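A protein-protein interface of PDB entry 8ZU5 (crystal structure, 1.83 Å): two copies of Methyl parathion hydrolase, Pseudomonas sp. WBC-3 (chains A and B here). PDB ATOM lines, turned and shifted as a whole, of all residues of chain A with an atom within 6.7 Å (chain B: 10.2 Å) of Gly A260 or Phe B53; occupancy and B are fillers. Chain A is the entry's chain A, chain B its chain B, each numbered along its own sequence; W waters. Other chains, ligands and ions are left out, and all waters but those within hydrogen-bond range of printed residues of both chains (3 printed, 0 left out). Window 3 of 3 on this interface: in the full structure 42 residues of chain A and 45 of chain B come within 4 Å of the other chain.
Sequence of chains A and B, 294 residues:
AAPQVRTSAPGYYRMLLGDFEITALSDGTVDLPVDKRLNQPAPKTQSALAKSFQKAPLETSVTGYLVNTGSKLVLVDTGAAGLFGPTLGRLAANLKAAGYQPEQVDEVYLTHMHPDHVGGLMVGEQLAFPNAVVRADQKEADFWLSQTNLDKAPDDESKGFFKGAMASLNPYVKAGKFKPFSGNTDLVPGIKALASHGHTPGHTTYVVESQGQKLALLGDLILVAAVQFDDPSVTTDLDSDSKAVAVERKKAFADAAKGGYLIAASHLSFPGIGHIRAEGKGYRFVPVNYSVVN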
ATOM      1  N   LYS A 214      -3.725  -2.174 -18.126  1.00  0.00           N
ATOM      2  CA  LYS A 214      -2.488  -2.494 -17.437  1.00  0.00           C
ATOM      3  C   LYS A 214      -1.769  -3.660 -18.128  1.00  0.00           C
ATOM      4  O   LYS A 214      -2.393  -4.561 -18.709  1.00  0.00           O
ATOM      5  CB  LYS A 214      -2.776  -2.822 -15.962  1.00  0.00           C
ATOM      6  CG  LYS A 214      -1.540  -3.000 -15.074  1.00  0.00           C
ATOM      7  CD  LYS A 214      -1.930  -3.427 -13.656  1.00  0.00           C
ATOM      8  CE  LYS A 214      -2.557  -2.309 -12.867  1.00  0.00           C
ATOM      9  NZ  LYS A 214      -2.797  -2.737 -11.454  1.00  0.00           N
ATOM     10  N   ASP A 255      -2.366 -11.906  -8.717  1.00  0.00           N
ATOM     11  CA  ASP A 255      -2.822 -10.542  -8.964  1.00  0.00           C
ATOM     12  C   ASP A 255      -3.298 -10.353 -10.400  1.00  0.00           C
ATOM     13  O   ASP A 255      -4.311  -9.679 -10.640  1.00  0.00           O
ATOM     14  CB  ASP A 255      -1.708  -9.547  -8.644  1.00  0.00           C
ATOM     15  CG  ASP A 255      -2.233  -8.124  -8.483  1.00  0.00           C
ATOM     16  OD1 ASP A 255      -2.928  -7.856  -7.485  1.00  0.00           O
ATOM     17  OD2 ASP A 255      -1.983  -7.276  -9.354  1.00  0.00           O
ATOM     18  N   ALA A 256      -2.585 -10.926 -11.378  1.00  0.00           N
ATOM     19  CA  ALA A 256      -3.038 -10.763 -12.751  1.00  0.00           C
ATOM     20  C   ALA A 256      -4.315 -11.560 -13.015  1.00  0.00           C
ATOM     21  O   ALA A 256      -5.173 -11.110 -13.786  1.00  0.00           O
ATOM     22  CB  ALA A 256      -1.927 -11.160 -13.720  1.00  0.00           C
ATOM     23  N   ALA A 257      -4.480 -12.720 -12.364  1.00  0.00           N
ATOM     24  CA  ALA A 257      -5.719 -13.466 -12.534  1.00  0.00           C
ATOM     25  C   ALA A 257      -6.890 -12.764 -11.857  1.00  0.00           C
ATOM     26  O   ALA A 257      -8.020 -12.814 -12.356  1.00  0.00           O
ATOM     27  CB  ALA A 257      -5.563 -14.883 -12.001  1.00  0.00           C
ATOM     28  N   LYS A 258      -6.650 -12.129 -10.704  1.00  0.00           N
ATOM     29  CA  LYS A 258      -7.696 -11.328 -10.077  1.00  0.00           C
ATOM     30  C   LYS A 258      -8.072 -10.132 -10.940  1.00  0.00           C
ATOM     31  O   LYS A 258      -9.261  -9.844 -11.135  1.00  0.00           O
ATOM     32  CB  LYS A 258      -7.234 -10.842  -8.705  1.00  0.00           C
ATOM     33  CG  LYS A 258      -7.034 -11.938  -7.678  1.00  0.00           C
ATOM     34  CD  LYS A 258      -6.527 -11.391  -6.345  1.00  0.00           C
ATOM     35  CE  LYS A 258      -6.330 -12.538  -5.369  1.00  0.00           C
ATOM     36  NZ  LYS A 258      -5.808 -12.143  -4.025  1.00  0.00           N
ATOM     37  N   GLY A 259      -7.068  -9.413 -11.453  1.00  0.00           N
ATOM     38  CA  GLY A 259      -7.290  -8.161 -12.147  1.00  0.00           C
ATOM     39  C   GLY A 259      -7.642  -8.348 -13.608  1.00  0.00           C
ATOM     40  O   GLY A 259      -8.225  -7.456 -14.234  1.00  0.00           O
ATOM     41  N   GLY A 260      -7.299  -9.509 -14.160  1.00  0.00           N
ATOM     42  CA  GLY A 260      -7.570  -9.761 -15.562  1.00  0.00           C
ATOM     43  C   GLY A 260      -6.855  -8.821 -16.494  1.00  0.00           C
ATOM     44  O   GLY A 260      -7.408  -8.450 -17.535  1.00  0.00           O
ATOM     45  N   TYR A 261      -5.636  -8.419 -16.146  1.00  0.00           N
ATOM     46  CA  TYR A 261      -4.816  -7.585 -17.015  1.00  0.00           C
ATOM     47  C   TYR A 261      -3.699  -8.424 -17.638  1.00  0.00           C
ATOM     48  O   TYR A 261      -3.466  -9.583 -17.266  1.00  0.00           O
ATOM     49  CB  TYR A 261      -4.297  -6.351 -16.228  1.00  0.00           C
ATOM     50  CG  TYR A 261      -3.483  -6.679 -14.987  1.00  0.00           C
ATOM     51  CD1 TYR A 261      -2.150  -7.090 -15.105  1.00  0.00           C
ATOM     52  CD2 TYR A 261      -4.038  -6.591 -13.696  1.00  0.00           C
ATOM     53  CE1 TYR A 261      -1.405  -7.416 -14.003  1.00  0.00           C
ATOM     54  CE2 TYR A 261      -3.269  -6.906 -12.568  1.00  0.00           C
ATOM     55  CZ  TYR A 261      -1.943  -7.314 -12.750  1.00  0.00           C
ATOM     56  OH  TYR A 261      -1.126  -7.650 -11.695  1.00  0.00           O
ATOM     57  N   LEU A 262      -3.032  -7.844 -18.642  1.00  0.00           N
ATOM     58  CA  LEU A 262      -2.019  -8.573 -19.389  1.00  0.00           C
ATOM     59  C   LEU A 262      -0.707  -8.615 -18.629  1.00  0.00           C
ATOM     60  O   LEU A 262      -0.359  -7.687 -17.902  1.00  0.00           O
ATOM     61  CB  LEU A 262      -1.780  -7.928 -20.753  1.00  0.00           C
ATOM     62  CG  LEU A 262      -2.857  -8.059 -21.829  1.00  0.00           C
ATOM     63  CD1 LEU A 262      -2.533  -7.154 -23.007  1.00  0.00           C
ATOM     64  CD2 LEU A 262      -2.896  -9.471 -22.318  1.00  0.00           C
ATOM     65  N   HIS A 275      -2.913 -13.108 -20.953  1.00  0.00           N
ATOM     66  CA  HIS A 275      -3.610 -13.070 -19.674  1.00  0.00           C
ATOM     67  C   HIS A 275      -3.331 -14.346 -18.881  1.00  0.00           C
ATOM     68  O   HIS A 275      -2.776 -15.322 -19.380  1.00  0.00           O
ATOM     69  CB  HIS A 275      -5.131 -12.924 -19.862  1.00  0.00           C
ATOM     70  CG  HIS A 275      -5.553 -11.631 -20.474  1.00  0.00           C
ATOM     71  ND1 HIS A 275      -5.699 -11.471 -21.836  1.00  0.00           N
ATOM     72  CD2 HIS A 275      -5.823 -10.427 -19.919  1.00  0.00           C
ATOM     73  CE1 HIS A 275      -6.061 -10.226 -22.090  1.00  0.00           C
ATOM     74  NE2 HIS A 275      -6.117  -9.564 -20.948  1.00  0.00           N
ATOM     75  N   ILE A 276      -3.791 -14.360 -17.640  1.00  0.00           N
ATOM     76  CA  ILE A 276      -3.549 -15.486 -16.753  1.00  0.00           C
ATOM     77  C   ILE A 276      -4.825 -15.733 -15.977  1.00  0.00           C
ATOM     78  O   ILE A 276      -5.463 -14.782 -15.519  1.00  0.00           O
ATOM     79  CB  ILE A 276      -2.363 -15.215 -15.800  1.00  0.00           C
ATOM     80  CG1 ILE A 276      -2.033 -16.437 -14.941  1.00  0.00           C
ATOM     81  CG2 ILE A 276      -2.648 -14.093 -14.895  1.00  0.00           C
ATOM     82  CD1 ILE A 276      -1.732 -17.612 -15.745  1.00  0.00           C
ATOM     83  N   ARG A 277      -5.222 -16.998 -15.854  1.00  0.00           N
ATOM     84  CA  ARG A 277      -6.321 -17.333 -14.961  1.00  0.00           C
ATOM     85  C   ARG A 277      -5.953 -18.520 -14.100  1.00  0.00           C
ATOM     86  O   ARG A 277      -5.150 -19.379 -14.476  1.00  0.00           O
ATOM     87  CB  ARG A 277      -7.650 -17.621 -15.685  1.00  0.00           C
ATOM     88  CG  ARG A 277      -7.569 -18.587 -16.814  1.00  0.00           C
ATOM     89  CD  ARG A 277      -8.948 -18.829 -17.392  1.00  0.00           C
ATOM     90  NE  ARG A 277      -9.133 -20.208 -17.810  1.00  0.00           N
ATOM     91  CZ  ARG A 277      -9.020 -20.606 -19.070  1.00  0.00           C
ATOM     92  NH1 ARG A 277      -8.708 -19.752 -20.038  1.00  0.00           N
ATOM     93  NH2 ARG A 277      -9.229 -21.888 -19.369  1.00  0.00           N
ATOM     94  N   ARG A 284      -3.307 -21.042 -15.946  1.00  0.00           N
ATOM     95  CA  ARG A 284      -3.249 -21.330 -17.403  1.00  0.00           C
ATOM     96  C   ARG A 284      -3.044 -19.995 -18.148  1.00  0.00           C
ATOM     97  O   ARG A 284      -3.899 -19.094 -17.983  1.00  0.00           O
ATOM     98  CB  ARG A 284      -4.535 -22.043 -17.838  1.00  0.00           C
ATOM     99  CG  ARG A 284      -4.960 -21.813 -19.281  1.00  0.00           C
ATOM    100  CD  ARG A 284      -5.691 -23.014 -19.853  1.00  0.00           C
ATOM    101  NE  ARG A 284      -4.815 -24.186 -19.947  1.00  0.00           N
ATOM    102  CZ  ARG A 284      -5.135 -25.403 -19.526  1.00  0.00           C
ATOM    103  NH1 ARG A 284      -6.159 -25.569 -18.708  1.00  0.00           N
ATOM    104  NH2 ARG A 284      -4.434 -26.448 -19.927  1.00  0.00           N
ATOM    105  N   VAL A 286      -3.071 -17.424 -21.193  1.00  0.00           N
ATOM    106  CA  VAL A 286      -3.875 -17.253 -22.391  1.00  0.00           C
ATOM    107  C   VAL A 286      -3.194 -16.205 -23.264  1.00  0.00           C
ATOM    108  O   VAL A 286      -3.287 -15.000 -22.981  1.00  0.00           O
ATOM    109  CB  VAL A 286      -5.322 -16.870 -22.047  1.00  0.00           C
ATOM    110  CG1 VAL A 286      -6.155 -16.772 -23.317  1.00  0.00           C
ATOM    111  CG2 VAL A 286      -5.954 -17.949 -21.095  1.00  0.00           C
ATOM    112  N   ASN A 289      -4.973 -12.316 -27.852  1.00  0.00           N
ATOM    113  CA  ASN A 289      -5.611 -12.455 -29.154  1.00  0.00           C
ATOM    114  C   ASN A 289      -4.887 -11.572 -30.169  1.00  0.00           C
ATOM    115  O   ASN A 289      -4.631 -10.393 -29.897  1.00  0.00           O
ATOM    116  CB  ASN A 289      -7.076 -12.031 -29.021  1.00  0.00           C
ATOM    117  CG  ASN A 289      -7.882 -12.278 -30.272  1.00  0.00           C
ATOM    118  OD1 ASN A 289      -7.839 -13.371 -30.842  1.00  0.00           O
ATOM    119  ND2 ASN A 289      -8.675 -11.288 -30.681  1.00  0.00           N
ATOM    120  N   THR B  45     -22.211 -18.122 -24.670  1.00  0.00           N
ATOM    121  CA  THR B  45     -21.066 -17.727 -25.481  1.00  0.00           C
ATOM    122  C   THR B  45     -20.331 -16.555 -24.842  1.00  0.00           C
ATOM    123  O   THR B  45     -19.092 -16.527 -24.778  1.00  0.00           O
ATOM    124  CB  THR B  45     -21.553 -17.363 -26.877  1.00  0.00           C
ATOM    125  OG1 THR B  45     -22.089 -18.521 -27.531  1.00  0.00           O
ATOM    126  CG2 THR B  45     -20.375 -16.764 -27.734  1.00  0.00           C
ATOM    127  N   GLN B  46     -21.089 -15.571 -24.373  1.00  0.00           N
ATOM    128  CA  GLN B  46     -20.529 -14.398 -23.709  1.00  0.00           C
ATOM    129  C   GLN B  46     -19.557 -14.818 -22.612  1.00  0.00           C
ATOM    130  O   GLN B  46     -18.413 -14.329 -22.539  1.00  0.00           O
ATOM    131  CB  GLN B  46     -21.703 -13.600 -23.133  1.00  0.00           C
ATOM    132  CG  GLN B  46     -21.436 -12.568 -22.053  1.00  0.00           C
ATOM    133  CD  GLN B  46     -22.690 -11.742 -21.754  1.00  0.00           C
ATOM    134  OE1 GLN B  46     -22.688 -10.885 -20.867  1.00  0.00           O
ATOM    135  NE2 GLN B  46     -23.791 -12.065 -22.443  1.00  0.00           N
ATOM    136  N   SER B  47     -20.007 -15.746 -21.752  1.00  0.00           N
ATOM    137  CA  SER B  47     -19.191 -16.213 -20.636  1.00  0.00           C
ATOM    138  C   SER B  47     -17.947 -16.970 -21.103  1.00  0.00           C
ATOM    139  O   SER B  47     -16.860 -16.772 -20.548  1.00  0.00           O
ATOM    140  CB  SER B  47     -20.052 -17.068 -19.690  1.00  0.00           C
ATOM    141  OG  SER B  47     -20.257 -18.403 -20.150  1.00  0.00           O
ATOM    142  N   ALA B  48     -18.079 -17.862 -22.092  1.00  0.00           N
ATOM    143  CA  ALA B  48     -16.888 -18.569 -22.584  1.00  0.00           C
ATOM    144  C   ALA B  48     -15.849 -17.590 -23.149  1.00  0.00           C
ATOM    145  O   ALA B  48     -14.641 -17.672 -22.840  1.00  0.00           O
ATOM    146  CB  ALA B  48     -17.297 -19.598 -23.636  1.00  0.00           C
ATOM    147  N   LEU B  49     -16.313 -16.623 -23.935  1.00  0.00           N
ATOM    148  CA  LEU B  49     -15.422 -15.569 -24.415  1.00  0.00           C
ATOM    149  C   LEU B  49     -14.730 -14.883 -23.243  1.00  0.00           C
ATOM    150  O   LEU B  49     -13.509 -14.704 -23.241  1.00  0.00           O
ATOM    151  CB  LEU B  49     -16.225 -14.556 -25.228  1.00  0.00           C
ATOM    152  CG  LEU B  49     -16.699 -14.951 -26.625  1.00  0.00           C
ATOM    153  CD1 LEU B  49     -17.065 -13.721 -27.443  1.00  0.00           C
ATOM    154  CD2 LEU B  49     -15.645 -15.784 -27.329  1.00  0.00           C
ATOM    155  N   ALA B  50     -15.492 -14.514 -22.226  1.00  0.00           N
ATOM    156  CA  ALA B  50     -14.909 -13.741 -21.102  1.00  0.00           C
ATOM    157  C   ALA B  50     -13.908 -14.589 -20.324  1.00  0.00           C
ATOM    158  O   ALA B  50     -12.956 -14.026 -19.777  1.00  0.00           O
ATOM    159  CB  ALA B  50     -16.012 -13.198 -20.224  1.00  0.00           C
ATOM    160  N   LYS B  51     -14.088 -15.903 -20.319  1.00  0.00           N
ATOM    161  CA  LYS B  51     -13.118 -16.800 -19.643  1.00  0.00           C
ATOM    162  C   LYS B  51     -11.769 -16.731 -20.375  1.00  0.00           C
ATOM    163  O   LYS B  51     -10.747 -16.997 -19.737  1.00  0.00           O
ATOM    164  CB  LYS B  51     -13.654 -18.232 -19.588  1.00  0.00           C
ATOM    165  CG  LYS B  51     -13.670 -18.885 -18.221  1.00  0.00           C
ATOM    166  CD  LYS B  51     -14.313 -20.265 -18.243  1.00  0.00           C
ATOM    167  CE  LYS B  51     -15.557 -20.331 -17.411  1.00  0.00           C
ATOM    168  NZ  LYS B  51     -15.881 -21.697 -16.989  1.00  0.00           N
ATOM    169  N   SER B  52     -11.793 -16.418 -21.671  1.00  0.00           N
ATOM    170  CA  SER B  52     -10.551 -16.326 -22.479  1.00  0.00           C
ATOM    171  C   SER B  52     -10.243 -14.842 -22.686  1.00  0.00           C
ATOM    172  O   SER B  52      -9.441 -14.533 -23.576  1.00  0.00           O
ATOM    173  CB  SER B  52     -10.702 -17.086 -23.762  1.00  0.00           C
ATOM    174  OG  SER B  52     -10.556 -18.482 -23.551  1.00  0.00           O
ATOM    175  N   PHE B  53     -10.917 -13.983 -21.923  1.00  0.00           N
ATOM    176  CA  PHE B  53     -10.675 -12.543 -21.940  1.00  0.00           C
ATOM    177  C   PHE B  53     -11.010 -11.916 -23.299  1.00  0.00           C
ATOM    178  O   PHE B  53     -10.302 -11.034 -23.793  1.00  0.00           O
ATOM    179  CB  PHE B  53      -9.236 -12.234 -21.503  1.00  0.00           C
ATOM    180  CG  PHE B  53      -8.858 -12.834 -20.146  1.00  0.00           C
ATOM    181  CD1 PHE B  53      -8.332 -14.111 -20.046  1.00  0.00           C
ATOM    182  CD2 PHE B  53      -9.041 -12.105 -18.982  1.00  0.00           C
ATOM    183  CE1 PHE B  53      -7.973 -14.625 -18.811  1.00  0.00           C
ATOM    184  CE2 PHE B  53      -8.705 -12.628 -17.746  1.00  0.00           C
ATOM    185  CZ  PHE B  53      -8.177 -13.889 -17.657  1.00  0.00           C
ATOM    186  N   GLN B  54     -12.146 -12.339 -23.869  1.00  0.00           N
ATOM    187  CA  GLN B  54     -12.711 -11.806 -25.107  1.00  0.00           C
ATOM    188  C   GLN B  54     -14.146 -11.383 -24.824  1.00  0.00           C
ATOM    189  O   GLN B  54     -14.741 -11.836 -23.846  1.00  0.00           O
ATOM    190  CB  GLN B  54     -12.659 -12.853 -26.238  1.00  0.00           C
ATOM    191  CG  GLN B  54     -11.321 -13.601 -26.355  1.00  0.00           C
ATOM    192  CD  GLN B  54     -11.337 -14.793 -27.328  1.00  0.00           C
ATOM    193  OE1 GLN B  54     -12.390 -15.240 -27.779  1.00  0.00           O
ATOM    194  NE2 GLN B  54     -10.153 -15.286 -27.669  1.00  0.00           N
ATOM    195  N   LYS B  55     -14.723 -10.522 -25.671  1.00  0.00           N
ATOM    196  CA  LYS B  55     -16.136 -10.184 -25.469  1.00  0.00           C
ATOM    197  C   LYS B  55     -16.682  -9.547 -26.748  1.00  0.00           C
ATOM    198  O   LYS B  55     -15.955  -9.378 -27.733  1.00  0.00           O
ATOM    199  CB  LYS B  55     -16.341  -9.259 -24.244  1.00  0.00           C
ATOM    200  CG  LYS B  55     -17.821  -8.958 -23.873  1.00  0.00           C
ATOM    201  CD  LYS B  55     -18.023  -8.101 -22.609  1.00  0.00           C
ATOM    202  CE  LYS B  55     -19.533  -7.884 -22.362  1.00  0.00           C
ATOM    203  NZ  LYS B  55     -19.865  -7.068 -21.153  1.00  0.00           N
ATOM    204  N   ALA B  56     -18.015  -9.261 -26.741  1.00  0.00           N
ATOM    205  CA  ALA B  56     -18.736  -8.380 -27.665  1.00  0.00           C
ATOM    206  C   ALA B  56     -18.495  -8.970 -29.042  1.00  0.00           C
ATOM    207  O   ALA B  56     -18.207 -10.173 -29.112  1.00  0.00           O
ATOM    208  CB  ALA B  56     -18.274  -6.926 -27.498  1.00  0.00           C
ATOM    209  N   PRO B  57     -18.644  -8.248 -30.155  1.00  0.00           N
ATOM    210  CA  PRO B  57     -18.052  -8.765 -31.393  1.00  0.00           C
ATOM    211  C   PRO B  57     -16.584  -9.102 -31.163  1.00  0.00           C
ATOM    212  O   PRO B  57     -15.856  -8.372 -30.485  1.00  0.00           O
ATOM    213  CB  PRO B  57     -18.228  -7.612 -32.377  1.00  0.00           C
ATOM    214  CG  PRO B  57     -19.535  -7.013 -31.972  1.00  0.00           C
ATOM    215  CD  PRO B  57     -19.644  -7.199 -30.464  1.00  0.00           C
ATOM    216  N   LEU B  58     -16.160 -10.228 -31.707  1.00  0.00           N
ATOM    217  CA  LEU B  58     -14.832 -10.759 -31.457  1.00  0.00           C
ATOM    218  C   LEU B  58     -13.922 -10.525 -32.660  1.00  0.00           C
ATOM    219  O   LEU B  58     -14.225 -10.979 -33.778  1.00  0.00           O
ATOM    220  CB  LEU B  58     -14.916 -12.254 -31.165  1.00  0.00           C
ATOM    221  CG  LEU B  58     -13.598 -13.021 -31.022  1.00  0.00           C
ATOM    222  CD1 LEU B  58     -12.674 -12.317 -30.014  1.00  0.00           C
ATOM    223  CD2 LEU B  58     -13.882 -14.490 -30.658  1.00  0.00           C
ATOM    224  N   GLU B  59     -12.769  -9.896 -32.421  1.00  0.00           N
ATOM    225  CA  GLU B  59     -11.800  -9.707 -33.504  1.00  0.00           C
ATOM    226  C   GLU B  59     -11.217 -11.057 -33.909  1.00  0.00           C
ATOM    227  O   GLU B  59     -10.517 -11.709 -33.125  1.00  0.00           O
ATOM    228  CB  GLU B  59     -10.692  -8.749 -33.075  1.00  0.00           C
ATOM    229  CG  GLU B  59      -9.504  -8.709 -34.016  1.00  0.00           C
ATOM    230  CD  GLU B  59      -8.552  -7.535 -33.749  1.00  0.00           C
ATOM    231  OE1 GLU B  59      -8.544  -6.988 -32.624  1.00  0.00           O
ATOM    232  OE2 GLU B  59      -7.790  -7.166 -34.665  1.00  0.00           O
ATOM    233  N   ALA B 225     -12.545 -20.543 -31.042  1.00  0.00           N
ATOM    234  CA  ALA B 225     -11.723 -21.358 -30.141  1.00  0.00           C
ATOM    235  C   ALA B 225     -12.211 -21.308 -28.697  1.00  0.00           C
ATOM    236  O   ALA B 225     -12.195 -22.329 -27.991  1.00  0.00           O
ATOM    237  CB  ALA B 225     -10.270 -20.886 -30.231  1.00  0.00           C
ATOM    238  N   ALA B 226     -12.617 -20.132 -28.223  1.00  0.00           N
ATOM    239  CA  ALA B 226     -12.991 -20.003 -26.818  1.00  0.00           C
ATOM    240  C   ALA B 226     -14.267 -20.774 -26.467  1.00  0.00           C
ATOM    241  O   ALA B 226     -14.605 -20.875 -25.287  1.00  0.00           O
ATOM    242  CB  ALA B 226     -13.116 -18.518 -26.465  1.00  0.00           C
ATOM    243  N   VAL B 227     -14.979 -21.325 -27.453  1.00  0.00           N
ATOM    244  CA  VAL B 227     -16.194 -22.107 -27.222  1.00  0.00           C
ATOM    245  C   VAL B 227     -16.010 -23.564 -27.630  1.00  0.00           C
ATOM    246  O   VAL B 227     -16.304 -24.479 -26.851  1.00  0.00           O
ATOM    247  CB  VAL B 227     -17.405 -21.476 -27.948  1.00  0.00           C
ATOM    248  CG1 VAL B 227     -18.675 -22.246 -27.678  1.00  0.00           C
ATOM    249  CG2 VAL B 227     -17.622 -20.085 -27.430  1.00  0.00           C
HETATM  250  O   HOH W   1      -7.385 -12.763 -33.765  1.00  0.00           O
HETATM  251  O   HOH W   2      -8.609  -8.421 -30.194  1.00  0.00           O
HETATM  252  O   HOH W   3      -7.156 -15.500 -28.578  1.00  0.00           O
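O of Lys B51 sits at hydrogen-bond distance from NH1 of Arg A277 (3.4 Å).
ND2 of Asn A289 sits at hydrogen-bond distance from O of Glu B59, at 3.1 Å.
The backbone carbonyl oxygen of His A275 sits at hydrogen-bond distance from the backbone NH of Val A286 (2.8 Å).
The backbone NH of Arg A284 sits at hydrogen-bond distance from the backbone carbonyl oxygen of Arg A277 (2.9 Å).
Among the printed residues, merely in contact across the chains: His A275 with Phe B53 (3.4 Å), Ile A276 with Phe B53 (3.6 Å), Gly A260 with Phe B53 (3.8 Å) and Val A286 with Ser B52 (3.98 Å).
No residue of chain B comes within 4 Å of Ala A256.
Of chain B, only Phe B53 (3.4 Å) comes within 4 Å of His A275.
Printed residues of chain B within 4 Å of Ile A276: Phe B53 (3.6 Å).
Arg A284 touches none of the printed residues of chain B.
Of the printed residues of chain B, Val A286 touches Ser B52 (3.98 Å).
Of the printed residues of chain A, Lys B51 touches Arg A277.
Gln B54 touches none of the printed residues of chain A.
The nearest residue of chain B that does not touch Gly A260 is Ala B50 (8.1 Å).
The nearest printed residue of chain A that does not touch Ser B52 is Arg A277 (4.2 Å).
Hydrophobic or aromatic side chains of chain B within 4 Å of the printed part of chain A: Phe B53.
Hydrophobic or aromatic side chains of chain A that line the printed part of chain B: His A275 and Val A286.
Among the printed residues, 6 pairs touch across the chains.
No position is printed for both chains.
Of the 6 pairs that touch across the chains among the printed residues, none has its exchanged pair printed and touching as well.
Water W2 lies within hydrogen-bond range of OE1 of Glu B59 and ND2 of Asn A289.
Water W1 bridges OD1 of Asn A289 (3.0 Å) and O of Glu B59 (3.4 Å).
Water W3 bridges NE2 of Gln B54 (3.1 Å) and OD1 of Asn A289 (3.2 Å).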
